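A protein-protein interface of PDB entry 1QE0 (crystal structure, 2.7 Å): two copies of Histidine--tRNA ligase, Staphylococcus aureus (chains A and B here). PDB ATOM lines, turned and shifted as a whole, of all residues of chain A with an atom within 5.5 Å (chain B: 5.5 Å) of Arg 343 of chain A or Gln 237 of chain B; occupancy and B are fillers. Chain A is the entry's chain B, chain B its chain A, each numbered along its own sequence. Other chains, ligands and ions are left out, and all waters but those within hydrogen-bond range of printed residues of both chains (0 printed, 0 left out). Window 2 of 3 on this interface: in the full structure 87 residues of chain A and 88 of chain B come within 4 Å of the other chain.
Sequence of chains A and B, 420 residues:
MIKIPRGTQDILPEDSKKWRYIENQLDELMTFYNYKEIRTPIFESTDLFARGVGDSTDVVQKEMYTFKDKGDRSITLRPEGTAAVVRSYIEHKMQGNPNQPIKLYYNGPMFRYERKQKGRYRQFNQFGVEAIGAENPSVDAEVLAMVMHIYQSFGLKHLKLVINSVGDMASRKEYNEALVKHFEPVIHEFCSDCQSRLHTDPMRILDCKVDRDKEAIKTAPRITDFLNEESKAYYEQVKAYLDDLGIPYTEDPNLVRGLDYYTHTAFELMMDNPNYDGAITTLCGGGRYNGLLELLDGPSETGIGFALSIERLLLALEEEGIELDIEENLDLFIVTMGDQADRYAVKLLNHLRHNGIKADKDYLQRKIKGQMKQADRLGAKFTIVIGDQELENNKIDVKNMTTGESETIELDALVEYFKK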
ATOM      1  N   GLY A 338     -13.644  -6.945 -20.259  1.00  0.00           N
ATOM      2  CA  GLY A 338     -12.941  -5.682 -20.161  1.00  0.00           C
ATOM      3  C   GLY A 338     -13.665  -4.540 -20.838  1.00  0.00           C
ATOM      4  O   GLY A 338     -14.597  -4.763 -21.610  1.00  0.00           O
ATOM      5  N   ASP A 339     -13.186  -3.321 -20.595  1.00  0.00           N
ATOM      6  CA  ASP A 339     -13.782  -2.100 -21.138  1.00  0.00           C
ATOM      7  C   ASP A 339     -14.018  -1.994 -22.658  1.00  0.00           C
ATOM      8  O   ASP A 339     -15.133  -1.722 -23.095  1.00  0.00           O
ATOM      9  CB  ASP A 339     -12.992  -0.893 -20.650  1.00  0.00           C
ATOM     10  CG  ASP A 339     -12.951  -0.798 -19.138  1.00  0.00           C
ATOM     11  OD1 ASP A 339     -13.961  -1.139 -18.505  1.00  0.00           O
ATOM     12  OD2 ASP A 339     -11.915  -0.379 -18.576  1.00  0.00           O
ATOM     13  N   GLN A 340     -12.973  -2.186 -23.457  1.00  0.00           N
ATOM     14  CA  GLN A 340     -13.090  -2.096 -24.911  1.00  0.00           C
ATOM     15  C   GLN A 340     -14.286  -2.920 -25.387  1.00  0.00           C
ATOM     16  O   GLN A 340     -15.234  -2.386 -25.951  1.00  0.00           O
ATOM     17  CB  GLN A 340     -11.781  -2.569 -25.585  1.00  0.00           C
ATOM     18  CG  GLN A 340     -11.748  -2.453 -27.118  1.00  0.00           C
ATOM     19  CD  GLN A 340     -10.416  -2.898 -27.732  1.00  0.00           C
ATOM     20  OE1 GLN A 340      -9.652  -2.080 -28.229  1.00  0.00           O
ATOM     21  NE2 GLN A 340     -10.154  -4.197 -27.722  1.00  0.00           N
ATOM     22  N   ALA A 341     -14.257  -4.210 -25.083  1.00  0.00           N
ATOM     23  CA  ALA A 341     -15.319  -5.129 -25.464  1.00  0.00           C
ATOM     24  C   ALA A 341     -16.674  -4.677 -24.930  1.00  0.00           C
ATOM     25  O   ALA A 341     -17.677  -4.710 -25.640  1.00  0.00           O
ATOM     26  CB  ALA A 341     -14.999  -6.506 -24.949  1.00  0.00           C
ATOM     27  N   ASP A 342     -16.693  -4.233 -23.682  1.00  0.00           N
ATOM     28  CA  ASP A 342     -17.922  -3.798 -23.067  1.00  0.00           C
ATOM     29  C   ASP A 342     -18.529  -2.554 -23.695  1.00  0.00           C
ATOM     30  O   ASP A 342     -19.748  -2.429 -23.810  1.00  0.00           O
ATOM     31  CB  ASP A 342     -17.710  -3.552 -21.601  1.00  0.00           C
ATOM     32  CG  ASP A 342     -18.946  -3.040 -20.946  1.00  0.00           C
ATOM     33  OD1 ASP A 342     -18.994  -1.827 -20.644  1.00  0.00           O
ATOM     34  OD2 ASP A 342     -19.893  -3.839 -20.794  1.00  0.00           O
ATOM     35  N   ARG A 343     -17.693  -1.607 -24.078  1.00  0.00           N
ATOM     36  CA  ARG A 343     -18.190  -0.386 -24.691  1.00  0.00           C
ATOM     37  C   ARG A 343     -18.669  -0.662 -26.106  1.00  0.00           C
ATOM     38  O   ARG A 343     -19.409   0.120 -26.697  1.00  0.00           O
ATOM     39  CB  ARG A 343     -17.120   0.709 -24.648  1.00  0.00           C
ATOM     40  CG  ARG A 343     -16.847   1.223 -23.223  1.00  0.00           C
ATOM     41  CD  ARG A 343     -15.955   2.441 -23.238  1.00  0.00           C
ATOM     42  NE  ARG A 343     -14.564   2.108 -23.523  1.00  0.00           N
ATOM     43  CZ  ARG A 343     -13.634   1.989 -22.584  1.00  0.00           C
ATOM     44  NH1 ARG A 343     -12.383   1.678 -22.914  1.00  0.00           N
ATOM     45  NH2 ARG A 343     -13.957   2.197 -21.309  1.00  0.00           N
ATOM     46  N   TYR A 344     -18.255  -1.798 -26.634  1.00  0.00           N
ATOM     47  CA  TYR A 344     -18.670  -2.237 -27.961  1.00  0.00           C
ATOM     48  C   TYR A 344     -20.077  -2.851 -27.866  1.00  0.00           C
ATOM     49  O   TYR A 344     -20.924  -2.664 -28.744  1.00  0.00           O
ATOM     50  CB  TYR A 344     -17.684  -3.279 -28.473  1.00  0.00           C
ATOM     51  CG  TYR A 344     -18.079  -3.842 -29.791  1.00  0.00           C
ATOM     52  CD1 TYR A 344     -17.787  -3.159 -30.969  1.00  0.00           C
ATOM     53  CD2 TYR A 344     -18.782  -5.036 -29.872  1.00  0.00           C
ATOM     54  CE1 TYR A 344     -18.190  -3.648 -32.192  1.00  0.00           C
ATOM     55  CE2 TYR A 344     -19.189  -5.533 -31.091  1.00  0.00           C
ATOM     56  CZ  TYR A 344     -18.890  -4.830 -32.247  1.00  0.00           C
ATOM     57  OH  TYR A 344     -19.314  -5.314 -33.458  1.00  0.00           O
ATOM     58  N   ALA A 345     -20.290  -3.604 -26.787  1.00  0.00           N
ATOM     59  CA  ALA A 345     -21.550  -4.274 -26.484  1.00  0.00           C
ATOM     60  C   ALA A 345     -22.669  -3.268 -26.362  1.00  0.00           C
ATOM     61  O   ALA A 345     -23.821  -3.628 -26.529  1.00  0.00           O
ATOM     62  CB  ALA A 345     -21.426  -5.050 -25.186  1.00  0.00           C
ATOM     63  N   VAL A 346     -22.341  -2.025 -25.999  1.00  0.00           N
ATOM     64  CA  VAL A 346     -23.360  -0.977 -25.880  1.00  0.00           C
ATOM     65  C   VAL A 346     -23.878  -0.537 -27.255  1.00  0.00           C
ATOM     66  O   VAL A 346     -25.082  -0.469 -27.444  1.00  0.00           O
ATOM     67  CB  VAL A 346     -22.903   0.219 -25.024  1.00  0.00           C
ATOM     68  CG1 VAL A 346     -23.931   1.343 -25.094  1.00  0.00           C
ATOM     69  CG2 VAL A 346     -22.725  -0.233 -23.585  1.00  0.00           C
ATOM     70  N   LYS A 347     -23.006  -0.295 -28.229  1.00  0.00           N
ATOM     71  CA  LYS A 347     -23.515   0.060 -29.562  1.00  0.00           C
ATOM     72  C   LYS A 347     -24.260  -1.159 -30.108  1.00  0.00           C
ATOM     73  O   LYS A 347     -25.325  -1.037 -30.703  1.00  0.00           O
ATOM     74  CB  LYS A 347     -22.398   0.405 -30.558  1.00  0.00           C
ATOM     75  CG  LYS A 347     -21.282   1.257 -30.000  1.00  0.00           C
ATOM     76  CD  LYS A 347     -20.140   1.371 -31.004  1.00  0.00           C
ATOM     77  CE  LYS A 347     -18.862   1.774 -30.264  1.00  0.00           C
ATOM     78  NZ  LYS A 347     -17.581   1.434 -30.943  1.00  0.00           N
ATOM     79  N   PRO B 137     -22.713   4.007 -16.242  1.00  0.00           N
ATOM     80  CA  PRO B 137     -22.905   4.791 -17.457  1.00  0.00           C
ATOM     81  C   PRO B 137     -23.583   4.002 -18.562  1.00  0.00           C
ATOM     82  O   PRO B 137     -24.504   4.491 -19.178  1.00  0.00           O
ATOM     83  CB  PRO B 137     -21.481   5.132 -17.852  1.00  0.00           C
ATOM     84  CG  PRO B 137     -20.841   5.379 -16.527  1.00  0.00           C
ATOM     85  CD  PRO B 137     -21.425   4.328 -15.606  1.00  0.00           C
ATOM     86  N   SER B 138     -23.179   2.763 -18.780  1.00  0.00           N
ATOM     87  CA  SER B 138     -23.781   1.988 -19.839  1.00  0.00           C
ATOM     88  C   SER B 138     -25.259   1.767 -19.599  1.00  0.00           C
ATOM     89  O   SER B 138     -25.995   1.555 -20.552  1.00  0.00           O
ATOM     90  CB  SER B 138     -23.075   0.660 -19.996  1.00  0.00           C
ATOM     91  OG  SER B 138     -23.159  -0.061 -18.785  1.00  0.00           O
ATOM     92  N   ALA B 233     -16.608  12.058 -14.808  1.00  0.00           N
ATOM     93  CA  ALA B 233     -16.214  11.009 -15.744  1.00  0.00           C
ATOM     94  C   ALA B 233     -17.381  10.103 -16.026  1.00  0.00           C
ATOM     95  O   ALA B 233     -17.413   9.438 -17.057  1.00  0.00           O
ATOM     96  CB  ALA B 233     -15.080  10.220 -15.207  1.00  0.00           C
ATOM     97  N   TYR B 234     -18.309  10.008 -15.077  1.00  0.00           N
ATOM     98  CA  TYR B 234     -19.504   9.197 -15.293  1.00  0.00           C
ATOM     99  C   TYR B 234     -20.239   9.924 -16.421  1.00  0.00           C
ATOM    100  O   TYR B 234     -20.506   9.349 -17.483  1.00  0.00           O
ATOM    101  CB  TYR B 234     -20.367   9.169 -14.033  1.00  0.00           C
ATOM    102  CG  TYR B 234     -21.532   8.205 -14.069  1.00  0.00           C
ATOM    103  CD1 TYR B 234     -22.450   8.194 -15.126  1.00  0.00           C
ATOM    104  CD2 TYR B 234     -21.726   7.318 -13.036  1.00  0.00           C
ATOM    105  CE1 TYR B 234     -23.521   7.318 -15.135  1.00  0.00           C
ATOM    106  CE2 TYR B 234     -22.792   6.438 -13.046  1.00  0.00           C
ATOM    107  CZ  TYR B 234     -23.678   6.436 -14.088  1.00  0.00           C
ATOM    108  OH  TYR B 234     -24.685   5.503 -14.069  1.00  0.00           O
ATOM    109  N   TYR B 235     -20.468  11.219 -16.202  1.00  0.00           N
ATOM    110  CA  TYR B 235     -21.152  12.071 -17.149  1.00  0.00           C
ATOM    111  C   TYR B 235     -20.453  12.049 -18.488  1.00  0.00           C
ATOM    112  O   TYR B 235     -21.113  11.999 -19.533  1.00  0.00           O
ATOM    113  CB  TYR B 235     -21.245  13.503 -16.622  1.00  0.00           C
ATOM    114  CG  TYR B 235     -21.959  14.464 -17.564  1.00  0.00           C
ATOM    115  CD1 TYR B 235     -21.428  15.723 -17.841  1.00  0.00           C
ATOM    116  CD2 TYR B 235     -23.175  14.118 -18.174  1.00  0.00           C
ATOM    117  CE1 TYR B 235     -22.080  16.610 -18.684  1.00  0.00           C
ATOM    118  CE2 TYR B 235     -23.832  15.007 -19.017  1.00  0.00           C
ATOM    119  CZ  TYR B 235     -23.282  16.244 -19.255  1.00  0.00           C
ATOM    120  OH  TYR B 235     -23.989  17.140 -20.005  1.00  0.00           O
ATOM    121  N   GLU B 236     -19.127  12.090 -18.478  1.00  0.00           N
ATOM    122  CA  GLU B 236     -18.413  12.067 -19.748  1.00  0.00           C
ATOM    123  C   GLU B 236     -18.591  10.722 -20.426  1.00  0.00           C
ATOM    124  O   GLU B 236     -18.532  10.648 -21.641  1.00  0.00           O
ATOM    125  CB  GLU B 236     -16.911  12.369 -19.619  1.00  0.00           C
ATOM    126  CG  GLU B 236     -16.489  13.688 -18.949  1.00  0.00           C
ATOM    127  CD  GLU B 236     -17.153  14.966 -19.472  1.00  0.00           C
ATOM    128  OE1 GLU B 236     -17.790  15.679 -18.642  1.00  0.00           O
ATOM    129  OE2 GLU B 236     -16.994  15.279 -20.683  1.00  0.00           O
ATOM    130  N   GLN B 237     -18.759   9.651 -19.652  1.00  0.00           N
ATOM    131  CA  GLN B 237     -18.963   8.327 -20.232  1.00  0.00           C
ATOM    132  C   GLN B 237     -20.364   8.231 -20.821  1.00  0.00           C
ATOM    133  O   GLN B 237     -20.532   7.704 -21.926  1.00  0.00           O
ATOM    134  CB  GLN B 237     -18.762   7.232 -19.199  1.00  0.00           C
ATOM    135  CG  GLN B 237     -18.778   5.839 -19.814  1.00  0.00           C
ATOM    136  CD  GLN B 237     -17.875   5.747 -21.032  1.00  0.00           C
ATOM    137  OE1 GLN B 237     -18.284   5.286 -22.097  1.00  0.00           O
ATOM    138  NE2 GLN B 237     -16.644   6.217 -20.887  1.00  0.00           N
ATOM    139  N   VAL B 238     -21.365   8.731 -20.085  1.00  0.00           N
ATOM    140  CA  VAL B 238     -22.741   8.745 -20.579  1.00  0.00           C
ATOM    141  C   VAL B 238     -22.738   9.421 -21.957  1.00  0.00           C
ATOM    142  O   VAL B 238     -23.137   8.809 -22.951  1.00  0.00           O
ATOM    143  CB  VAL B 238     -23.674   9.489 -19.622  1.00  0.00           C
ATOM    144  CG1 VAL B 238     -25.050   9.669 -20.244  1.00  0.00           C
ATOM    145  CG2 VAL B 238     -23.770   8.710 -18.306  1.00  0.00           C
ATOM    146  N   LYS B 239     -22.206  10.639 -22.046  1.00  0.00           N
ATOM    147  CA  LYS B 239     -22.165  11.334 -23.339  1.00  0.00           C
ATOM    148  C   LYS B 239     -21.291  10.614 -24.346  1.00  0.00           C
ATOM    149  O   LYS B 239     -21.544  10.670 -25.531  1.00  0.00           O
ATOM    150  CB  LYS B 239     -21.697  12.777 -23.200  1.00  0.00           C
ATOM    151  CG  LYS B 239     -22.543  13.560 -22.270  1.00  0.00           C
ATOM    152  CD  LYS B 239     -22.055  14.968 -22.206  1.00  0.00           C
ATOM    153  CE  LYS B 239     -20.730  15.061 -21.506  1.00  0.00           C
ATOM    154  NZ  LYS B 239     -20.358  16.480 -21.330  1.00  0.00           N
ATOM    155  N   ALA B 240     -20.256   9.939 -23.875  1.00  0.00           N
ATOM    156  CA  ALA B 240     -19.382   9.205 -24.772  1.00  0.00           C
ATOM    157  C   ALA B 240     -20.278   8.218 -25.478  1.00  0.00           C
ATOM    158  O   ALA B 240     -20.335   8.178 -26.706  1.00  0.00           O
ATOM    159  CB  ALA B 240     -18.349   8.463 -23.998  1.00  0.00           C
ATOM    160  N   TYR B 241     -21.020   7.460 -24.680  1.00  0.00           N
ATOM    161  CA  TYR B 241     -21.937   6.453 -25.189  1.00  0.00           C
ATOM    162  C   TYR B 241     -22.949   7.020 -26.157  1.00  0.00           C
ATOM    163  O   TYR B 241     -23.230   6.415 -27.196  1.00  0.00           O
ATOM    164  CB  TYR B 241     -22.643   5.774 -24.026  1.00  0.00           C
ATOM    165  CG  TYR B 241     -21.773   4.725 -23.392  1.00  0.00           C
ATOM    166  CD1 TYR B 241     -21.098   3.810 -24.188  1.00  0.00           C
ATOM    167  CD2 TYR B 241     -21.678   4.599 -22.011  1.00  0.00           C
ATOM    168  CE1 TYR B 241     -20.369   2.793 -23.635  1.00  0.00           C
ATOM    169  CE2 TYR B 241     -20.934   3.570 -21.445  1.00  0.00           C
ATOM    170  CZ  TYR B 241     -20.291   2.669 -22.283  1.00  0.00           C
ATOM    171  OH  TYR B 241     -19.589   1.590 -21.803  1.00  0.00           O
ATOM    172  N   LEU B 242     -23.516   8.173 -25.806  1.00  0.00           N
ATOM    173  CA  LEU B 242     -24.478   8.839 -26.675  1.00  0.00           C
ATOM    174  C   LEU B 242     -23.788   9.124 -27.993  1.00  0.00           C
ATOM    175  O   LEU B 242     -24.342   8.879 -29.046  1.00  0.00           O
ATOM    176  CB  LEU B 242     -24.978  10.137 -26.043  1.00  0.00           C
ATOM    177  CG  LEU B 242     -26.290  10.025 -25.252  1.00  0.00           C
ATOM    178  CD1 LEU B 242     -26.636   8.529 -24.982  1.00  0.00           C
ATOM    179  CD2 LEU B 242     -26.209  10.904 -23.965  1.00  0.00           C
ATOM    180  N   ASP B 244     -21.275   7.477 -29.227  1.00  0.00           N
ATOM    181  CA  ASP B 244     -21.081   6.143 -29.823  1.00  0.00           C
ATOM    182  C   ASP B 244     -22.319   5.727 -30.599  1.00  0.00           C
ATOM    183  O   ASP B 244     -22.247   5.383 -31.772  1.00  0.00           O
ATOM    184  CB  ASP B 244     -20.937   5.088 -28.733  1.00  0.00           C
ATOM    185  CG  ASP B 244     -19.549   4.990 -28.159  1.00  0.00           C
ATOM    186  OD1 ASP B 244     -19.062   5.983 -27.565  1.00  0.00           O
ATOM    187  OD2 ASP B 244     -18.975   3.875 -28.222  1.00  0.00           O
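Of the 13 printed residues of chain B, 4 touch a printed residue of chain A. Of the 10 printed residues of chain A, 4 touch a printed residue of chain B. Hydrophobic or aromatic side chains of chain A within 4 Å of the printed part of chain B: Val 346. Among the printed residues, 6 pairs touch across the chains. Among the printed residues, Asp or Glu carboxylates within 4 Å of a Lys or Arg side-chain nitrogen of the other chain: Lys 347 of chain A with Asp 244 of chain B (3.9 Å).
Among the printed residues, merely in contact across the chains: Arg 343 of chain A with Tyr 241 of chain B, Asp 342 of chain A with Tyr 241 of chain B, Val 346 of chain A with Ser 138 of chain B, Val 346 of chain A with Tyr 241 of chain B and Arg 343 of chain A with Gln 237 of chain B.
Of chain B, only Gln 237 (3.8 Å) and Tyr 241 (3.1 Å) come within 4 Å of Arg 343 of chain A. Gln 237 of chain B touches one residue of chain A. Printed residues of chain B within 4 Å of Val 346 of chain A: Ser 138 (3.7 Å) and Tyr 241 (3.8 Å). Of the printed residues of chain B, Asp 342 of chain A touches Tyr 241 (3.7 Å). The nearest residue of chain B that does not touch Arg 343 of chain A is Asp 244 of chain B (4.1 Å). The nearest printed residue of chain A that does not touch Gln 237 of chain B is Val 346 of chain A (7.2 Å).
No position is printed for both chains.
O of Ala 240 of chain B lies close to OD1 of Asp 244 of chain B.
OD2 of Asp 244 of chain B lies within salt-bridge range of NZ of Lys 347 of chain A (3.9 Å).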
